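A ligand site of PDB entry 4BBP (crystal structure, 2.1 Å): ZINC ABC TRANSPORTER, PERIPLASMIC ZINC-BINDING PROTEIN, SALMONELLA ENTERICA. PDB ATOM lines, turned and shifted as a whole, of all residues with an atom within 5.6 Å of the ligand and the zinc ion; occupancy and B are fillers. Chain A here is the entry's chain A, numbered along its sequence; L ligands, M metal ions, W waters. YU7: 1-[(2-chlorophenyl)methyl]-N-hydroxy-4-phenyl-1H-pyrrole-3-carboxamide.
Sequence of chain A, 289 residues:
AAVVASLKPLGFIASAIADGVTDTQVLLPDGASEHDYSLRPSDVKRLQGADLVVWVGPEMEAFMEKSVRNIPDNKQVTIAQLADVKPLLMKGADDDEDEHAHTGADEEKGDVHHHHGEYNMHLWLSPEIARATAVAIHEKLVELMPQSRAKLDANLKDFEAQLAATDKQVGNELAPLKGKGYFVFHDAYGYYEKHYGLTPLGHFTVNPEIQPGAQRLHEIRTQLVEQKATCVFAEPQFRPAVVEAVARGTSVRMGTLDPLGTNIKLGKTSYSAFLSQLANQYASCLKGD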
ATOM      1  N   LEU A   7      30.265  29.087   6.203  1.00  0.00           N
ATOM      2  CA  LEU A   7      28.931  28.935   5.644  1.00  0.00           C
ATOM      3  C   LEU A   7      27.909  29.117   6.752  1.00  0.00           C
ATOM      4  O   LEU A   7      28.193  28.856   7.916  1.00  0.00           O
ATOM      5  CB  LEU A   7      28.780  27.540   5.019  1.00  0.00           C
ATOM      6  CG  LEU A   7      29.695  27.175   3.838  1.00  0.00           C
ATOM      7  CD1 LEU A   7      29.803  25.667   3.625  1.00  0.00           C
ATOM      8  CD2 LEU A   7      29.250  27.882   2.531  1.00  0.00           C
ATOM      9  N   LEU A  28      30.657  34.411   3.929  1.00  0.00           N
ATOM     10  CA  LEU A  28      30.123  34.629   2.589  1.00  0.00           C
ATOM     11  C   LEU A  28      28.588  34.699   2.560  1.00  0.00           C
ATOM     12  O   LEU A  28      27.913  34.050   3.346  1.00  0.00           O
ATOM     13  CB  LEU A  28      30.633  33.507   1.656  1.00  0.00           C
ATOM     14  CG  LEU A  28      30.200  32.029   1.769  1.00  0.00           C
ATOM     15  CD1 LEU A  28      29.312  31.694   2.960  1.00  0.00           C
ATOM     16  CD2 LEU A  28      29.571  31.497   0.485  1.00  0.00           C
ATOM     17  N   ASP A  30      24.894  33.843   1.028  1.00  0.00           N
ATOM     18  CA  ASP A  30      24.374  32.530   0.660  1.00  0.00           C
ATOM     19  C   ASP A  30      24.543  32.203  -0.829  1.00  0.00           C
ATOM     20  O   ASP A  30      24.832  31.051  -1.193  1.00  0.00           O
ATOM     21  CB  ASP A  30      22.913  32.396   1.083  1.00  0.00           C
ATOM     22  CG  ASP A  30      22.742  32.407   2.592  1.00  0.00           C
ATOM     23  OD1 ASP A  30      23.641  31.938   3.318  1.00  0.00           O
ATOM     24  OD2 ASP A  30      21.694  32.892   3.057  1.00  0.00           O
ATOM     25  N   GLY A  31      24.388  33.204  -1.681  1.00  0.00           N
ATOM     26  CA  GLY A  31      24.424  33.014  -3.128  1.00  0.00           C
ATOM     27  C   GLY A  31      25.743  32.556  -3.723  1.00  0.00           C
ATOM     28  O   GLY A  31      25.805  32.209  -4.904  1.00  0.00           O
ATOM     29  N   ALA A  32      26.804  32.564  -2.912  1.00  0.00           N
ATOM     30  CA  ALA A  32      28.121  32.173  -3.368  1.00  0.00           C
ATOM     31  C   ALA A  32      28.225  30.641  -3.519  1.00  0.00           C
ATOM     32  O   ALA A  32      27.244  29.925  -3.313  1.00  0.00           O
ATOM     33  CB  ALA A  32      29.177  32.710  -2.429  1.00  0.00           C
ATOM     34  N   SER A  33      29.421  30.173  -3.902  1.00  0.00           N
ATOM     35  CA  SER A  33      29.710  28.733  -4.093  1.00  0.00           C
ATOM     36  C   SER A  33      31.154  28.370  -3.701  1.00  0.00           C
ATOM     37  O   SER A  33      31.767  29.060  -2.877  1.00  0.00           O
ATOM     38  CB  SER A  33      29.402  28.302  -5.535  1.00  0.00           C
ATOM     39  OG  SER A  33      30.421  28.762  -6.421  1.00  0.00           O
ATOM     40  N   GLU A  34      31.705  27.307  -4.308  1.00  0.00           N
ATOM     41  CA  GLU A  34      32.973  26.698  -3.870  1.00  0.00           C
ATOM     42  C   GLU A  34      34.206  26.844  -4.795  1.00  0.00           C
ATOM     43  O   GLU A  34      35.345  26.894  -4.301  1.00  0.00           O
ATOM     44  CB  GLU A  34      32.761  25.220  -3.530  1.00  0.00           C
ATOM     45  CG  GLU A  34      32.757  24.255  -4.737  1.00  0.00           C
ATOM     46  CD  GLU A  34      34.094  23.535  -4.991  1.00  0.00           C
ATOM     47  OE1 GLU A  34      34.837  23.251  -4.022  1.00  0.00           O
ATOM     48  OE2 GLU A  34      34.394  23.209  -6.157  1.00  0.00           O
ATOM     49  N   MET A  60      35.524  21.171   0.207  1.00  0.00           N
ATOM     50  CA  MET A  60      34.295  21.933   0.143  1.00  0.00           C
ATOM     51  C   MET A  60      34.636  23.390  -0.230  1.00  0.00           C
ATOM     52  O   MET A  60      34.558  23.757  -1.387  1.00  0.00           O
ATOM     53  CB  MET A  60      33.492  21.761   1.456  1.00  0.00           C
ATOM     54  CG  MET A  60      32.180  22.521   1.587  1.00  0.00           C
ATOM     55  SD  MET A  60      30.986  22.419   0.227  1.00  0.00           S
ATOM     56  CE  MET A  60      30.336  20.768   0.330  1.00  0.00           C
ATOM     57  N   PHE A  63      38.136  27.425  -2.226  1.00  0.00           N
ATOM     58  CA  PHE A  63      38.541  28.814  -2.372  1.00  0.00           C
ATOM     59  C   PHE A  63      39.227  29.418  -1.138  1.00  0.00           C
ATOM     60  O   PHE A  63      39.878  30.454  -1.246  1.00  0.00           O
ATOM     61  CB  PHE A  63      37.327  29.681  -2.764  1.00  0.00           C
ATOM     62  CG  PHE A  63      36.240  29.716  -1.715  1.00  0.00           C
ATOM     63  CD1 PHE A  63      36.287  30.625  -0.664  1.00  0.00           C
ATOM     64  CD2 PHE A  63      35.154  28.846  -1.782  1.00  0.00           C
ATOM     65  CE1 PHE A  63      35.291  30.663   0.304  1.00  0.00           C
ATOM     66  CE2 PHE A  63      34.151  28.884  -0.806  1.00  0.00           C
ATOM     67  CZ  PHE A  63      34.235  29.791   0.237  1.00  0.00           C
ATOM     68  N   HIS A 114      32.731  20.961  -5.475  1.00  0.00           N
ATOM     69  CA  HIS A 114      32.779  20.211  -4.220  1.00  0.00           C
ATOM     70  C   HIS A 114      32.013  18.893  -4.312  1.00  0.00           C
ATOM     71  O   HIS A 114      31.967  18.127  -3.348  1.00  0.00           O
ATOM     72  CB  HIS A 114      32.240  21.057  -3.058  1.00  0.00           C
ATOM     73  CG  HIS A 114      30.797  21.445  -3.188  1.00  0.00           C
ATOM     74  ND1 HIS A 114      30.398  22.654  -3.702  1.00  0.00           N
ATOM     75  CD2 HIS A 114      29.660  20.790  -2.848  1.00  0.00           C
ATOM     76  CE1 HIS A 114      29.080  22.724  -3.683  1.00  0.00           C
ATOM     77  NE2 HIS A 114      28.610  21.614  -3.162  1.00  0.00           N
ATOM     78  N   HIS A 115      31.396  18.651  -5.475  1.00  0.00           N
ATOM     79  CA  HIS A 115      30.651  17.428  -5.728  1.00  0.00           C
ATOM     80  C   HIS A 115      31.516  16.380  -6.427  1.00  0.00           C
ATOM     81  O   HIS A 115      31.101  15.216  -6.551  1.00  0.00           O
ATOM     82  CB  HIS A 115      29.392  17.717  -6.554  1.00  0.00           C
ATOM     83  CG  HIS A 115      28.283  18.306  -5.755  1.00  0.00           C
ATOM     84  ND1 HIS A 115      27.331  17.536  -5.124  1.00  0.00           N
ATOM     85  CD2 HIS A 115      27.971  19.598  -5.465  1.00  0.00           C
ATOM     86  CE1 HIS A 115      26.479  18.321  -4.492  1.00  0.00           C
ATOM     87  NE2 HIS A 115      26.847  19.577  -4.672  1.00  0.00           N
ATOM     88  N   HIS A 122      28.670  17.977   2.389  1.00  0.00           N
ATOM     89  CA  HIS A 122      27.628  18.842   2.951  1.00  0.00           C
ATOM     90  C   HIS A 122      27.392  18.431   4.400  1.00  0.00           C
ATOM     91  O   HIS A 122      26.283  18.011   4.762  1.00  0.00           O
ATOM     92  CB  HIS A 122      26.324  18.785   2.158  1.00  0.00           C
ATOM     93  CG  HIS A 122      26.502  18.962   0.687  1.00  0.00           C
ATOM     94  ND1 HIS A 122      26.904  17.931  -0.146  1.00  0.00           N
ATOM     95  CD2 HIS A 122      26.356  20.049  -0.109  1.00  0.00           C
ATOM     96  CE1 HIS A 122      26.996  18.377  -1.384  1.00  0.00           C
ATOM     97  NE2 HIS A 122      26.655  19.650  -1.392  1.00  0.00           N
ATOM     98  N   TRP A 124      27.164  19.792   7.355  1.00  0.00           N
ATOM     99  CA  TRP A 124      26.282  20.475   8.300  1.00  0.00           C
ATOM    100  C   TRP A 124      24.888  19.852   8.358  1.00  0.00           C
ATOM    101  O   TRP A 124      24.114  20.129   9.280  1.00  0.00           O
ATOM    102  CB  TRP A 124      26.185  21.974   7.954  1.00  0.00           C
ATOM    103  CG  TRP A 124      25.677  22.246   6.575  1.00  0.00           C
ATOM    104  CD1 TRP A 124      24.379  22.466   6.207  1.00  0.00           C
ATOM    105  CD2 TRP A 124      26.448  22.318   5.360  1.00  0.00           C
ATOM    106  NE1 TRP A 124      24.288  22.677   4.848  1.00  0.00           N
ATOM    107  CE2 TRP A 124      25.544  22.601   4.300  1.00  0.00           C
ATOM    108  CE3 TRP A 124      27.815  22.194   5.070  1.00  0.00           C
ATOM    109  CZ2 TRP A 124      25.961  22.746   2.961  1.00  0.00           C
ATOM    110  CZ3 TRP A 124      28.236  22.332   3.747  1.00  0.00           C
ATOM    111  CH2 TRP A 124      27.302  22.619   2.702  1.00  0.00           C
ATOM    112  N   HIS A 186      19.801  18.378  -6.186  1.00  0.00           N
ATOM    113  CA  HIS A 186      21.086  18.600  -5.502  1.00  0.00           C
ATOM    114  C   HIS A 186      21.413  17.385  -4.663  1.00  0.00           C
ATOM    115  O   HIS A 186      20.639  16.998  -3.780  1.00  0.00           O
ATOM    116  CB  HIS A 186      20.967  19.858  -4.649  1.00  0.00           C
ATOM    117  CG  HIS A 186      22.252  20.322  -4.037  1.00  0.00           C
ATOM    118  ND1 HIS A 186      22.284  21.141  -2.927  1.00  0.00           N
ATOM    119  CD2 HIS A 186      23.544  20.094  -4.364  1.00  0.00           C
ATOM    120  CE1 HIS A 186      23.530  21.395  -2.600  1.00  0.00           C
ATOM    121  NE2 HIS A 186      24.329  20.767  -3.453  1.00  0.00           N
ATOM    122  N   ASP A 187      22.555  16.752  -4.923  1.00  0.00           N
ATOM    123  CA  ASP A 187      22.985  15.601  -4.133  1.00  0.00           C
ATOM    124  C   ASP A 187      23.672  16.086  -2.857  1.00  0.00           C
ATOM    125  O   ASP A 187      24.905  16.035  -2.734  1.00  0.00           O
ATOM    126  CB  ASP A 187      23.917  14.700  -4.960  1.00  0.00           C
ATOM    127  CG  ASP A 187      24.332  13.442  -4.209  1.00  0.00           C
ATOM    128  OD1 ASP A 187      23.479  12.849  -3.524  1.00  0.00           O
ATOM    129  OD2 ASP A 187      25.509  13.048  -4.318  1.00  0.00           O
ATOM    130  N   ALA A 188      22.879  16.583  -1.916  1.00  0.00           N
ATOM    131  CA  ALA A 188      23.418  17.164  -0.683  1.00  0.00           C
ATOM    132  C   ALA A 188      22.912  16.471   0.590  1.00  0.00           C
ATOM    133  O   ALA A 188      23.681  16.301   1.552  1.00  0.00           O
ATOM    134  CB  ALA A 188      23.077  18.649  -0.629  1.00  0.00           C
ATOM    135  N   GLU A 235      15.578  23.944  -4.796  1.00  0.00           N
ATOM    136  CA  GLU A 235      16.182  24.783  -3.776  1.00  0.00           C
ATOM    137  C   GLU A 235      15.832  26.244  -4.084  1.00  0.00           C
ATOM    138  O   GLU A 235      15.346  26.529  -5.185  1.00  0.00           O
ATOM    139  CB  GLU A 235      17.701  24.539  -3.737  1.00  0.00           C
ATOM    140  CG  GLU A 235      18.039  23.104  -3.383  1.00  0.00           C
ATOM    141  CD  GLU A 235      19.497  22.886  -3.032  1.00  0.00           C
ATOM    142  OE1 GLU A 235      20.357  23.659  -3.490  1.00  0.00           O
ATOM    143  OE2 GLU A 235      19.780  21.924  -2.303  1.00  0.00           O
ATOM    144  N   PRO A 236      16.051  27.176  -3.133  1.00  0.00           N
ATOM    145  CA  PRO A 236      15.557  28.553  -3.309  1.00  0.00           C
ATOM    146  C   PRO A 236      16.038  29.284  -4.560  1.00  0.00           C
ATOM    147  O   PRO A 236      15.337  30.140  -5.056  1.00  0.00           O
ATOM    148  CB  PRO A 236      16.059  29.266  -2.042  1.00  0.00           C
ATOM    149  CG  PRO A 236      16.132  28.154  -1.017  1.00  0.00           C
ATOM    150  CD  PRO A 236      16.666  26.982  -1.798  1.00  0.00           C
ATOM    151  N   GLN A 237      17.221  28.941  -5.052  1.00  0.00           N
ATOM    152  CA  GLN A 237      17.821  29.644  -6.184  1.00  0.00           C
ATOM    153  C   GLN A 237      17.276  29.207  -7.557  1.00  0.00           C
ATOM    154  O   GLN A 237      17.567  29.859  -8.568  1.00  0.00           O
ATOM    155  CB  GLN A 237      19.351  29.543  -6.135  1.00  0.00           C
ATOM    156  CG  GLN A 237      19.949  28.164  -6.513  1.00  0.00           C
ATOM    157  CD  GLN A 237      19.948  27.159  -5.356  1.00  0.00           C
ATOM    158  OE1 GLN A 237      20.580  26.104  -5.455  1.00  0.00           O
ATOM    159  NE2 GLN A 237      19.264  27.494  -4.265  1.00  0.00           N
ATOM    160  N   ASP A 258      15.890  24.091   1.596  1.00  0.00           N
ATOM    161  CA  ASP A 258      16.913  25.095   1.755  1.00  0.00           C
ATOM    162  C   ASP A 258      18.030  24.551   2.644  1.00  0.00           C
ATOM    163  O   ASP A 258      17.903  24.547   3.867  1.00  0.00           O
ATOM    164  CB  ASP A 258      16.322  26.393   2.321  1.00  0.00           C
ATOM    165  CG  ASP A 258      17.364  27.490   2.492  1.00  0.00           C
ATOM    166  OD1 ASP A 258      18.531  27.314   2.070  1.00  0.00           O
ATOM    167  OD2 ASP A 258      17.022  28.537   3.070  1.00  0.00           O
ATOM    168  N   PRO A 259      19.135  24.086   2.016  1.00  0.00           N
ATOM    169  CA  PRO A 259      20.214  23.408   2.749  1.00  0.00           C
ATOM    170  C   PRO A 259      21.095  24.386   3.547  1.00  0.00           C
ATOM    171  O   PRO A 259      21.986  23.948   4.283  1.00  0.00           O
ATOM    172  CB  PRO A 259      21.028  22.768   1.625  1.00  0.00           C
ATOM    173  CG  PRO A 259      20.877  23.717   0.473  1.00  0.00           C
ATOM    174  CD  PRO A 259      19.466  24.254   0.588  1.00  0.00           C
ATOM    175  N   LEU A 260      20.834  25.679   3.398  1.00  0.00           N
ATOM    176  CA  LEU A 260      21.597  26.693   4.119  1.00  0.00           C
ATOM    177  C   LEU A 260      20.781  27.450   5.186  1.00  0.00           C
ATOM    178  O   LEU A 260      21.330  28.262   5.910  1.00  0.00           O
ATOM    179  CB  LEU A 260      22.239  27.692   3.149  1.00  0.00           C
ATOM    180  CG  LEU A 260      23.259  27.205   2.117  1.00  0.00           C
ATOM    181  CD1 LEU A 260      23.485  28.340   1.135  1.00  0.00           C
ATOM    182  CD2 LEU A 260      24.597  26.777   2.744  1.00  0.00           C
ATOM    183  N   THR A 262      18.773  29.881   4.811  1.00  0.00           N
ATOM    184  CA  THR A 262      18.966  31.299   4.475  1.00  0.00           C
ATOM    185  C   THR A 262      18.128  32.287   5.329  1.00  0.00           C
ATOM    186  O   THR A 262      18.597  33.385   5.644  1.00  0.00           O
ATOM    187  CB  THR A 262      18.648  31.575   2.972  1.00  0.00           C
ATOM    188  OG1 THR A 262      17.304  31.159   2.675  1.00  0.00           O
ATOM    189  CG2 THR A 262      19.627  30.823   2.067  1.00  0.00           C
HETATM  190 CL   YU7 L   1      19.878  28.201  -0.383  1.00  0.00          CL
HETATM  191  C10 YU7 L   1      20.834  28.900  -1.734  1.00  0.00           C
HETATM  192  C9  YU7 L   1      20.686  30.251  -2.047  1.00  0.00           C
HETATM  193  C8  YU7 L   1      21.422  30.809  -3.097  1.00  0.00           C
HETATM  194  C7  YU7 L   1      22.310  30.008  -3.819  1.00  0.00           C
HETATM  195  C6  YU7 L   1      22.465  28.659  -3.501  1.00  0.00           C
HETATM  196  C5  YU7 L   1      21.731  28.092  -2.449  1.00  0.00           C
HETATM  197  C4  YU7 L   1      21.866  26.620  -2.079  1.00  0.00           C
HETATM  198  N2  YU7 L   1      23.234  26.086  -2.165  1.00  0.00           N
HETATM  199  C3  YU7 L   1      23.548  24.909  -2.713  1.00  0.00           C
HETATM  200  C11 YU7 L   1      24.373  26.657  -1.714  1.00  0.00           C
HETATM  201  C12 YU7 L   1      25.465  25.841  -1.970  1.00  0.00           C
HETATM  202  C2  YU7 L   1      24.921  24.730  -2.597  1.00  0.00           C
HETATM  203  C1  YU7 L   1      25.738  23.589  -3.078  1.00  0.00           C
HETATM  204  N1  YU7 L   1      25.939  23.545  -4.402  1.00  0.00           N
HETATM  205  O2  YU7 L   1      26.277  22.383  -5.089  1.00  0.00           O
HETATM  206  O1  YU7 L   1      26.206  22.770  -2.276  1.00  0.00           O
HETATM  207  C13 YU7 L   1      26.815  26.114  -1.655  1.00  0.00           C
HETATM  208  C18 YU7 L   1      27.842  25.205  -1.964  1.00  0.00           C
HETATM  209  C17 YU7 L   1      29.172  25.473  -1.641  1.00  0.00           C
HETATM  210  C16 YU7 L   1      29.493  26.667  -1.004  1.00  0.00           C
HETATM  211  C15 YU7 L   1      28.479  27.580  -0.696  1.00  0.00           C
HETATM  212  C14 YU7 L   1      27.152  27.303  -1.017  1.00  0.00           C
HETATM  213 ZN    ZN M   1      26.447  20.969  -3.113  1.00  0.00          ZN
HETATM  214  O   HOH W   1      26.695  29.962   0.681  1.00  0.00           O
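CD2 of Leu 7 touches C15 of the ligand, 3.3 Å away. O of Asp 30 touches C7 of the ligand, 3.8 Å away. Gly 31 touches the ligand (CA to C8, 3.7 Å). Ala 32 touches the ligand. Ser 33 touches the ligand (C to C16, 3.6 Å). Glu 235 touches the ligand (OE1 to C3, 3.5 Å). Pro 236 touches the ligand. Gln 237 touches the ligand. Asp 258 touches the ligand. Pro 259 touches the ligand. Leu 260 touches the ligand (CD1 to C11, 3.4 Å). Thr 262 touches the ligand. Hydrophobic or aromatic side chains within 4 Å of the ligand: Leu 7, His 114, His 115, His 122, His 186, Pro 236, Pro 259 and Leu 260. The nearest printed residue that does not touch the ligand is Met 60 (4.01 Å).
O1 of the ligand is bound to the zinc ion, 2.0 Å away. NE2 of His 115 binds the zinc ion (2.1 Å). The zinc ion is bound by a ring nitrogen (NE2) of His 186, at 2.2 Å. The zinc ion is bound by NE2 of His 122. The zinc ion is bound by NE2 of His 114, at 2.3 Å. The zinc ion is bound by an oxygen (O2) of the ligand, 2.4 Å away.
Four residues have an atom within 4 Å of the zinc ion: His 114, His 115, His 122 and His 186.
The backbone carbonyl oxygen (O) of Pro 259 lies within hydrogen-bond range of the indole nitrogen (NE1) of Trp 124 (2.7 Å). The backbone NH of His 114 is in hydrogen-bond range of the side-chain carboxylate of Glu 34 (2.9 Å). A ring nitrogen (ND1) of His 186 is in hydrogen-bond range of the side-chain carboxylate (OE2) of Glu 235, 2.7 Å away. The side-chain carboxylate (OD1) of Asp 258 lies close to the backbone NH (N) of Leu 260 (3.1 Å). OD2 of Asp 258 sits at hydrogen-bond distance from OG1 of Thr 262 (2.7 Å). The side-chain amide oxygen of Gln 237 lies close to the side-chain carboxylate of Glu 235.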
